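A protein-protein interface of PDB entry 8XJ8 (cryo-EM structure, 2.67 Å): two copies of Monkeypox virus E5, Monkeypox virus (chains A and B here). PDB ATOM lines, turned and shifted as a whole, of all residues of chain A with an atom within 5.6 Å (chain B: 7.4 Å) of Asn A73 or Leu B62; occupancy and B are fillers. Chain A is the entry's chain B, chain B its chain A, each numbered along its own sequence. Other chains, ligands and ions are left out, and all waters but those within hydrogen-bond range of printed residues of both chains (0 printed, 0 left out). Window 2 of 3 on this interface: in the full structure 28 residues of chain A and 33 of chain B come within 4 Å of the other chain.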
ATOM      1  N   ASN A   2       9.643 -20.694   2.747  1.00  0.00           N
ATOM      2  CA  ASN A   2       8.762 -20.563   3.903  1.00  0.00           C
ATOM      3  C   ASN A   2       8.361 -21.928   4.449  1.00  0.00           C
ATOM      4  O   ASN A   2       8.675 -22.264   5.589  1.00  0.00           O
ATOM      5  CB  ASN A   2       7.516 -19.756   3.537  1.00  0.00           C
ATOM      6  CG  ASN A   2       6.723 -19.324   4.755  1.00  0.00           C
ATOM      7  OD1 ASN A   2       7.251 -18.671   5.654  1.00  0.00           O
ATOM      8  ND2 ASN A   2       5.446 -19.685   4.789  1.00  0.00           N
ATOM      9  N   LEU A   4       9.302 -24.977   3.119  1.00  0.00           N
ATOM     10  CA  LEU A   4      10.526 -25.766   3.169  1.00  0.00           C
ATOM     11  C   LEU A   4      11.455 -25.300   4.281  1.00  0.00           C
ATOM     12  O   LEU A   4      12.130 -26.129   4.902  1.00  0.00           O
ATOM     13  CB  LEU A   4      11.242 -25.706   1.820  1.00  0.00           C
ATOM     14  CG  LEU A   4      10.466 -26.297   0.641  1.00  0.00           C
ATOM     15  CD1 LEU A   4      11.246 -26.149  -0.651  1.00  0.00           C
ATOM     16  CD2 LEU A   4      10.125 -27.754   0.897  1.00  0.00           C
ATOM     17  N   PHE A   5      11.494 -23.994   4.551  1.00  0.00           N
ATOM     18  CA  PHE A   5      12.244 -23.497   5.698  1.00  0.00           C
ATOM     19  C   PHE A   5      11.668 -24.033   7.003  1.00  0.00           C
ATOM     20  O   PHE A   5      12.419 -24.379   7.921  1.00  0.00           O
ATOM     21  CB  PHE A   5      12.251 -21.969   5.698  1.00  0.00           C
ATOM     22  CG  PHE A   5      13.157 -21.370   6.732  1.00  0.00           C
ATOM     23  CD1 PHE A   5      14.504 -21.194   6.471  1.00  0.00           C
ATOM     24  CD2 PHE A   5      12.661 -20.982   7.965  1.00  0.00           C
ATOM     25  CE1 PHE A   5      15.340 -20.643   7.421  1.00  0.00           C
ATOM     26  CE2 PHE A   5      13.491 -20.432   8.918  1.00  0.00           C
ATOM     27  CZ  PHE A   5      14.831 -20.261   8.645  1.00  0.00           C
ATOM     28  N   ALA A   8      12.809 -27.627   7.322  1.00  0.00           N
ATOM     29  CA  ALA A   8      14.210 -27.684   7.727  1.00  0.00           C
ATOM     30  C   ALA A   8      14.379 -27.323   9.197  1.00  0.00           C
ATOM     31  O   ALA A   8      15.169 -27.949   9.912  1.00  0.00           O
ATOM     32  CB  ALA A   8      15.048 -26.758   6.849  1.00  0.00           C
ATOM     33  N   LYS A  68      16.784 -31.011  -1.704  1.00  0.00           N
ATOM     34  CA  LYS A  68      18.042 -30.273  -1.750  1.00  0.00           C
ATOM     35  C   LYS A  68      17.889 -28.865  -1.191  1.00  0.00           C
ATOM     36  O   LYS A  68      18.822 -28.340  -0.574  1.00  0.00           O
ATOM     37  CB  LYS A  68      18.566 -30.225  -3.184  1.00  0.00           C
ATOM     38  CG  LYS A  68      19.256 -31.504  -3.628  1.00  0.00           C
ATOM     39  CD  LYS A  68      19.427 -31.542  -5.135  1.00  0.00           C
ATOM     40  CE  LYS A  68      19.444 -32.970  -5.651  1.00  0.00           C
ATOM     41  NZ  LYS A  68      18.920 -33.064  -7.042  1.00  0.00           N
ATOM     42  N   THR A  69      16.729 -28.237  -1.395  1.00  0.00           N
ATOM     43  CA  THR A  69      16.470 -26.941  -0.779  1.00  0.00           C
ATOM     44  C   THR A  69      16.479 -27.045   0.741  1.00  0.00           C
ATOM     45  O   THR A  69      17.072 -26.203   1.430  1.00  0.00           O
ATOM     46  CB  THR A  69      15.131 -26.389  -1.272  1.00  0.00           C
ATOM     47  OG1 THR A  69      15.214 -26.118  -2.676  1.00  0.00           O
ATOM     48  CG2 THR A  69      14.768 -25.115  -0.535  1.00  0.00           C
ATOM     49  N   VAL A  70      15.837 -28.082   1.282  1.00  0.00           N
ATOM     50  CA  VAL A  70      15.847 -28.304   2.723  1.00  0.00           C
ATOM     51  C   VAL A  70      17.261 -28.603   3.206  1.00  0.00           C
ATOM     52  O   VAL A  70      17.667 -28.165   4.288  1.00  0.00           O
ATOM     53  CB  VAL A  70      14.864 -29.431   3.090  1.00  0.00           C
ATOM     54  CG1 VAL A  70      14.956 -29.771   4.567  1.00  0.00           C
ATOM     55  CG2 VAL A  70      13.446 -29.035   2.721  1.00  0.00           C
ATOM     56  N   GLU A  71      18.036 -29.346   2.411  1.00  0.00           N
ATOM     57  CA  GLU A  71      19.419 -29.625   2.784  1.00  0.00           C
ATOM     58  C   GLU A  71      20.244 -28.348   2.853  1.00  0.00           C
ATOM     59  O   GLU A  71      21.056 -28.174   3.769  1.00  0.00           O
ATOM     60  CB  GLU A  71      20.045 -30.609   1.799  1.00  0.00           C
ATOM     61  CG  GLU A  71      21.470 -30.996   2.156  1.00  0.00           C
ATOM     62  CD  GLU A  71      22.189 -31.693   1.024  1.00  0.00           C
ATOM     63  OE1 GLU A  71      21.620 -31.776  -0.084  1.00  0.00           O
ATOM     64  OE2 GLU A  71      23.327 -32.160   1.242  1.00  0.00           O
ATOM     65  N   ALA A  72      20.061 -27.445   1.887  1.00  0.00           N
ATOM     66  CA  ALA A  72      20.772 -26.170   1.915  1.00  0.00           C
ATOM     67  C   ALA A  72      20.350 -25.331   3.116  1.00  0.00           C
ATOM     68  O   ALA A  72      21.191 -24.705   3.777  1.00  0.00           O
ATOM     69  CB  ALA A  72      20.533 -25.407   0.615  1.00  0.00           C
ATOM     70  N   ASN A  73      19.049 -25.314   3.416  1.00  0.00           N
ATOM     71  CA  ASN A  73      18.566 -24.585   4.583  1.00  0.00           C
ATOM     72  C   ASN A  73      19.182 -25.129   5.866  1.00  0.00           C
ATOM     73  O   ASN A  73      19.565 -24.360   6.755  1.00  0.00           O
ATOM     74  CB  ASN A  73      17.042 -24.658   4.650  1.00  0.00           C
ATOM     75  CG  ASN A  73      16.372 -23.552   3.868  1.00  0.00           C
ATOM     76  OD1 ASN A  73      16.926 -22.467   3.709  1.00  0.00           O
ATOM     77  ND2 ASN A  73      15.172 -23.823   3.371  1.00  0.00           N
ATOM     78  N   ILE A  74      19.275 -26.454   5.983  1.00  0.00           N
ATOM     79  CA  ILE A  74      19.906 -27.064   7.149  1.00  0.00           C
ATOM     80  C   ILE A  74      21.386 -26.708   7.206  1.00  0.00           C
ATOM     81  O   ILE A  74      21.920 -26.379   8.272  1.00  0.00           O
ATOM     82  CB  ILE A  74      19.688 -28.588   7.135  1.00  0.00           C
ATOM     83  CG1 ILE A  74      18.232 -28.925   7.456  1.00  0.00           C
ATOM     84  CG2 ILE A  74      20.622 -29.279   8.116  1.00  0.00           C
ATOM     85  CD1 ILE A  74      17.881 -30.373   7.226  1.00  0.00           C
ATOM     86  N   ARG A  75      22.072 -26.767   6.062  1.00  0.00           N
ATOM     87  CA  ARG A  75      23.502 -26.483   6.031  1.00  0.00           C
ATOM     88  C   ARG A  75      23.803 -25.048   6.431  1.00  0.00           C
ATOM     89  O   ARG A  75      24.853 -24.778   7.023  1.00  0.00           O
ATOM     90  CB  ARG A  75      24.061 -26.772   4.639  1.00  0.00           C
ATOM     91  CG  ARG A  75      24.512 -28.205   4.443  1.00  0.00           C
ATOM     92  CD  ARG A  75      25.461 -28.331   3.266  1.00  0.00           C
ATOM     93  NE  ARG A  75      25.415 -29.664   2.679  1.00  0.00           N
ATOM     94  CZ  ARG A  75      26.388 -30.558   2.775  1.00  0.00           C
ATOM     95  NH1 ARG A  75      27.509 -30.293   3.424  1.00  0.00           N
ATOM     96  NH2 ARG A  75      26.233 -31.751   2.207  1.00  0.00           N
ATOM     97  N   ASP A  76      22.905 -24.115   6.118  1.00  0.00           N
ATOM     98  CA  ASP A  76      23.085 -22.735   6.549  1.00  0.00           C
ATOM     99  C   ASP A  76      22.773 -22.521   8.025  1.00  0.00           C
ATOM    100  O   ASP A  76      23.135 -21.474   8.571  1.00  0.00           O
ATOM    101  CB  ASP A  76      22.215 -21.799   5.707  1.00  0.00           C
ATOM    102  CG  ASP A  76      22.880 -21.399   4.409  1.00  0.00           C
ATOM    103  OD1 ASP A  76      24.092 -21.656   4.257  1.00  0.00           O
ATOM    104  OD2 ASP A  76      22.191 -20.829   3.537  1.00  0.00           O
ATOM    105  N   MET A  77      22.122 -23.480   8.683  1.00  0.00           N
ATOM    106  CA  MET A  77      21.745 -23.347  10.084  1.00  0.00           C
ATOM    107  C   MET A  77      22.793 -23.886  11.049  1.00  0.00           C
ATOM    108  O   MET A  77      22.752 -23.541  12.235  1.00  0.00           O
ATOM    109  CB  MET A  77      20.423 -24.070  10.350  1.00  0.00           C
ATOM    110  CG  MET A  77      19.174 -23.291   9.988  1.00  0.00           C
ATOM    111  SD  MET A  77      17.852 -24.404   9.469  1.00  0.00           S
ATOM    112  CE  MET A  77      16.442 -23.307   9.508  1.00  0.00           C
ATOM    113  N   LEU B  47      21.706 -15.664   6.704  1.00  0.00           N
ATOM    114  CA  LEU B  47      20.580 -16.274   7.403  1.00  0.00           C
ATOM    115  C   LEU B  47      20.499 -15.798   8.850  1.00  0.00           C
ATOM    116  O   LEU B  47      19.406 -15.536   9.364  1.00  0.00           O
ATOM    117  CB  LEU B  47      20.688 -17.797   7.343  1.00  0.00           C
ATOM    118  CG  LEU B  47      19.490 -18.581   7.879  1.00  0.00           C
ATOM    119  CD1 LEU B  47      18.199 -18.090   7.250  1.00  0.00           C
ATOM    120  CD2 LEU B  47      19.672 -20.067   7.640  1.00  0.00           C
ATOM    121  N   ARG B  50      19.194 -11.927   9.525  1.00  0.00           N
ATOM    122  CA  ARG B  50      17.917 -11.504   8.960  1.00  0.00           C
ATOM    123  C   ARG B  50      17.004 -10.835   9.982  1.00  0.00           C
ATOM    124  O   ARG B  50      16.069 -10.133   9.586  1.00  0.00           O
ATOM    125  CB  ARG B  50      17.199 -12.701   8.334  1.00  0.00           C
ATOM    126  CG  ARG B  50      16.548 -13.634   9.338  1.00  0.00           C
ATOM    127  CD  ARG B  50      15.986 -14.867   8.655  1.00  0.00           C
ATOM    128  NE  ARG B  50      15.190 -15.682   9.566  1.00  0.00           N
ATOM    129  CZ  ARG B  50      15.692 -16.592  10.390  1.00  0.00           C
ATOM    130  NH1 ARG B  50      16.991 -16.828  10.451  1.00  0.00           N
ATOM    131  NH2 ARG B  50      14.867 -17.281  11.172  1.00  0.00           N
ATOM    132  N   TYR B  57      11.983  -7.618   4.358  1.00  0.00           N
ATOM    133  CA  TYR B  57      13.283  -8.086   3.898  1.00  0.00           C
ATOM    134  C   TYR B  57      13.675  -9.434   4.482  1.00  0.00           C
ATOM    135  O   TYR B  57      14.448 -10.166   3.856  1.00  0.00           O
ATOM    136  CB  TYR B  57      14.369  -7.061   4.241  1.00  0.00           C
ATOM    137  CG  TYR B  57      14.454  -5.897   3.279  1.00  0.00           C
ATOM    138  CD1 TYR B  57      13.442  -5.652   2.362  1.00  0.00           C
ATOM    139  CD2 TYR B  57      15.545  -5.039   3.292  1.00  0.00           C
ATOM    140  CE1 TYR B  57      13.516  -4.591   1.483  1.00  0.00           C
ATOM    141  CE2 TYR B  57      15.627  -3.974   2.417  1.00  0.00           C
ATOM    142  CZ  TYR B  57      14.609  -3.755   1.515  1.00  0.00           C
ATOM    143  OH  TYR B  57      14.686  -2.696   0.642  1.00  0.00           O
ATOM    144  N   SER B  58      13.163  -9.776   5.667  1.00  0.00           N
ATOM    145  CA  SER B  58      13.500 -11.057   6.280  1.00  0.00           C
ATOM    146  C   SER B  58      12.868 -12.224   5.536  1.00  0.00           C
ATOM    147  O   SER B  58      13.453 -13.312   5.483  1.00  0.00           O
ATOM    148  CB  SER B  58      13.066 -11.068   7.745  1.00  0.00           C
ATOM    149  OG  SER B  58      13.805 -10.128   8.502  1.00  0.00           O
ATOM    150  N   SER B  59      11.677 -12.027   4.966  1.00  0.00           N
ATOM    151  CA  SER B  59      11.011 -13.109   4.249  1.00  0.00           C
ATOM    152  C   SER B  59      11.766 -13.497   2.984  1.00  0.00           C
ATOM    153  O   SER B  59      11.731 -14.663   2.578  1.00  0.00           O
ATOM    154  CB  SER B  59       9.576 -12.709   3.909  1.00  0.00           C
ATOM    155  OG  SER B  59       9.551 -11.677   2.940  1.00  0.00           O
ATOM    156  N   GLU B  60      12.447 -12.541   2.349  1.00  0.00           N
ATOM    157  CA  GLU B  60      13.213 -12.841   1.145  1.00  0.00           C
ATOM    158  C   GLU B  60      14.432 -13.706   1.431  1.00  0.00           C
ATOM    159  O   GLU B  60      14.968 -14.320   0.504  1.00  0.00           O
ATOM    160  CB  GLU B  60      13.654 -11.544   0.464  1.00  0.00           C
ATOM    161  CG  GLU B  60      12.509 -10.653   0.016  1.00  0.00           C
ATOM    162  CD  GLU B  60      11.863 -11.135  -1.266  1.00  0.00           C
ATOM    163  OE1 GLU B  60      12.588 -11.326  -2.263  1.00  0.00           O
ATOM    164  OE2 GLU B  60      10.628 -11.324  -1.275  1.00  0.00           O
ATOM    165  N   LEU B  61      14.878 -13.770   2.683  1.00  0.00           N
ATOM    166  CA  LEU B  61      16.094 -14.483   3.044  1.00  0.00           C
ATOM    167  C   LEU B  61      15.833 -15.917   3.488  1.00  0.00           C
ATOM    168  O   LEU B  61      16.768 -16.603   3.909  1.00  0.00           O
ATOM    169  CB  LEU B  61      16.843 -13.723   4.141  1.00  0.00           C
ATOM    170  CG  LEU B  61      17.358 -12.338   3.743  1.00  0.00           C
ATOM    171  CD1 LEU B  61      18.267 -11.771   4.819  1.00  0.00           C
ATOM    172  CD2 LEU B  61      18.077 -12.394   2.405  1.00  0.00           C
ATOM    173  N   LEU B  62      14.588 -16.383   3.411  1.00  0.00           N
ATOM    174  CA  LEU B  62      14.274 -17.770   3.724  1.00  0.00           C
ATOM    175  C   LEU B  62      14.459 -18.701   2.536  1.00  0.00           C
ATOM    176  O   LEU B  62      14.355 -19.920   2.701  1.00  0.00           O
ATOM    177  CB  LEU B  62      12.836 -17.887   4.243  1.00  0.00           C
ATOM    178  CG  LEU B  62      12.522 -17.237   5.592  1.00  0.00           C
ATOM    179  CD1 LEU B  62      11.228 -17.792   6.158  1.00  0.00           C
ATOM    180  CD2 LEU B  62      13.664 -17.437   6.571  1.00  0.00           C
ATOM    181  N   CYS B  63      14.729 -18.158   1.348  1.00  0.00           N
ATOM    182  CA  CYS B  63      14.957 -18.961   0.158  1.00  0.00           C
ATOM    183  C   CYS B  63      16.450 -19.104  -0.078  1.00  0.00           C
ATOM    184  O   CYS B  63      17.140 -18.085  -0.231  1.00  0.00           O
ATOM    185  CB  CYS B  63      14.292 -18.320  -1.054  1.00  0.00           C
ATOM    186  SG  CYS B  63      14.209 -19.384  -2.512  1.00  0.00           S
ATOM    187  N   PRO B  64      16.996 -20.322  -0.100  1.00  0.00           N
ATOM    188  CA  PRO B  64      18.440 -20.469  -0.340  1.00  0.00           C
ATOM    189  C   PRO B  64      18.885 -19.962  -1.700  1.00  0.00           C
ATOM    190  O   PRO B  64      20.058 -19.609  -1.863  1.00  0.00           O
ATOM    191  CB  PRO B  64      18.665 -21.981  -0.195  1.00  0.00           C
ATOM    192  CG  PRO B  64      17.333 -22.589  -0.437  1.00  0.00           C
ATOM    193  CD  PRO B  64      16.338 -21.621   0.116  1.00  0.00           C
ATOM    194  N   ARG B  65      17.987 -19.924  -2.687  1.00  0.00           N
ATOM    195  CA  ARG B  65      18.352 -19.388  -3.994  1.00  0.00           C
ATOM    196  C   ARG B  65      18.554 -17.878  -3.932  1.00  0.00           C
ATOM    197  O   ARG B  65      19.454 -17.339  -4.585  1.00  0.00           O
ATOM    198  CB  ARG B  65      17.284 -19.755  -5.027  1.00  0.00           C
ATOM    199  CG  ARG B  65      17.057 -18.709  -6.110  1.00  0.00           C
ATOM    200  CD  ARG B  65      15.630 -18.745  -6.640  1.00  0.00           C
ATOM    201  NE  ARG B  65      14.677 -18.183  -5.692  1.00  0.00           N
ATOM    202  CZ  ARG B  65      13.372 -18.419  -5.710  1.00  0.00           C
ATOM    203  NH1 ARG B  65      12.823 -19.198  -6.627  1.00  0.00           N
ATOM    204  NH2 ARG B  65      12.598 -17.862  -4.783  1.00  0.00           N
ATOM    205  N   LYS B  66      17.733 -17.182  -3.145  1.00  0.00           N
ATOM    206  CA  LYS B  66      17.860 -15.736  -3.019  1.00  0.00           C
ATOM    207  C   LYS B  66      19.060 -15.332  -2.172  1.00  0.00           C
ATOM    208  O   LYS B  66      19.656 -14.278  -2.419  1.00  0.00           O
ATOM    209  CB  LYS B  66      16.579 -15.147  -2.431  1.00  0.00           C
ATOM    210  CG  LYS B  66      15.417 -15.142  -3.404  1.00  0.00           C
ATOM    211  CD  LYS B  66      14.133 -14.703  -2.733  1.00  0.00           C
ATOM    212  CE  LYS B  66      13.012 -14.569  -3.745  1.00  0.00           C
ATOM    213  NZ  LYS B  66      11.750 -14.107  -3.109  1.00  0.00           N
ATOM    214  N   ARG B  67      19.422 -16.141  -1.173  1.00  0.00           N
ATOM    215  CA  ARG B  67      20.596 -15.831  -0.365  1.00  0.00           C
ATOM    216  C   ARG B  67      21.875 -15.897  -1.185  1.00  0.00           C
ATOM    217  O   ARG B  67      22.831 -15.168  -0.900  1.00  0.00           O
ATOM    218  CB  ARG B  67      20.685 -16.779   0.831  1.00  0.00           C
ATOM    219  CG  ARG B  67      19.606 -16.565   1.874  1.00  0.00           C
ATOM    220  CD  ARG B  67      19.878 -17.375   3.130  1.00  0.00           C
ATOM    221  NE  ARG B  67      19.988 -18.802   2.857  1.00  0.00           N
ATOM    222  CZ  ARG B  67      19.123 -19.715   3.274  1.00  0.00           C
ATOM    223  NH1 ARG B  67      18.053 -19.384   3.977  1.00  0.00           N
ATOM    224  NH2 ARG B  67      19.336 -20.994   2.978  1.00  0.00           N
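The guanidinium group (NH2) of Arg B67 lies within hydrogen-bond range of the side-chain amide oxygen (OD1) of Asn A73, 2.9 Å away. The guanidinium group (NH2) of Arg B67 lies within salt-bridge range of the side-chain carboxylate (OD2) of Asp A76 (2.9 Å).
The guanidinium group of Arg B50 sits at hydrogen-bond distance from the backbone carbonyl oxygen of Leu B47 (2.9 Å). O of Arg B50 lies within hydrogen-bond range of OG of Ser B58. O of Leu B61 sits at hydrogen-bond distance from NH1 of Arg B67 (3.1 Å).
Among the printed residues, pairs that only touch across the chains: Phe A5 with Leu B47, Phe A5 with Arg B50, Phe A5 with Leu B62, Thr A69 with Pro B64, Ala A72 with Pro B64, Asn A73 with Leu B62, Asn A73 with Pro B64 and Asp A76 with Leu B47.
Of the printed residues of chain B, Thr A69 touches Pro B64. Of chain B, only Leu B62, Pro B64 and Arg B67 come within 4 Å of Asn A73. Of the printed residues of chain B, Asp A76 touches Leu B47 and Arg B67. Ser B59 touches none of the printed residues of chain A. Leu B62 touches just these residues of chain A: Phe A5 (3.7 Å) and Asn A73 (3.8 Å). Cys B63 touches none of the printed residues of chain A. The nearest printed residue of chain A that does not touch Leu B47 is Met A77 (4.02 Å).
Printed residues of chain B that touch a printed residue of chain A: Leu B47, Arg B50, Leu B62, Pro B64 and Arg B67. Hydrophobic or aromatic side chains of chain A that line the printed part of chain B: Phe A5 and Ala A72. Among the printed residues, Asp or Glu carboxylates within 4 Å of a Lys or Arg side-chain nitrogen of the other chain: Asp A76 with Arg B67 (2.9 Å).
No position is printed for both chains. Of the 10 pairs that touch across the chains among the printed residues, none has its exchanged pair printed and touching as well.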
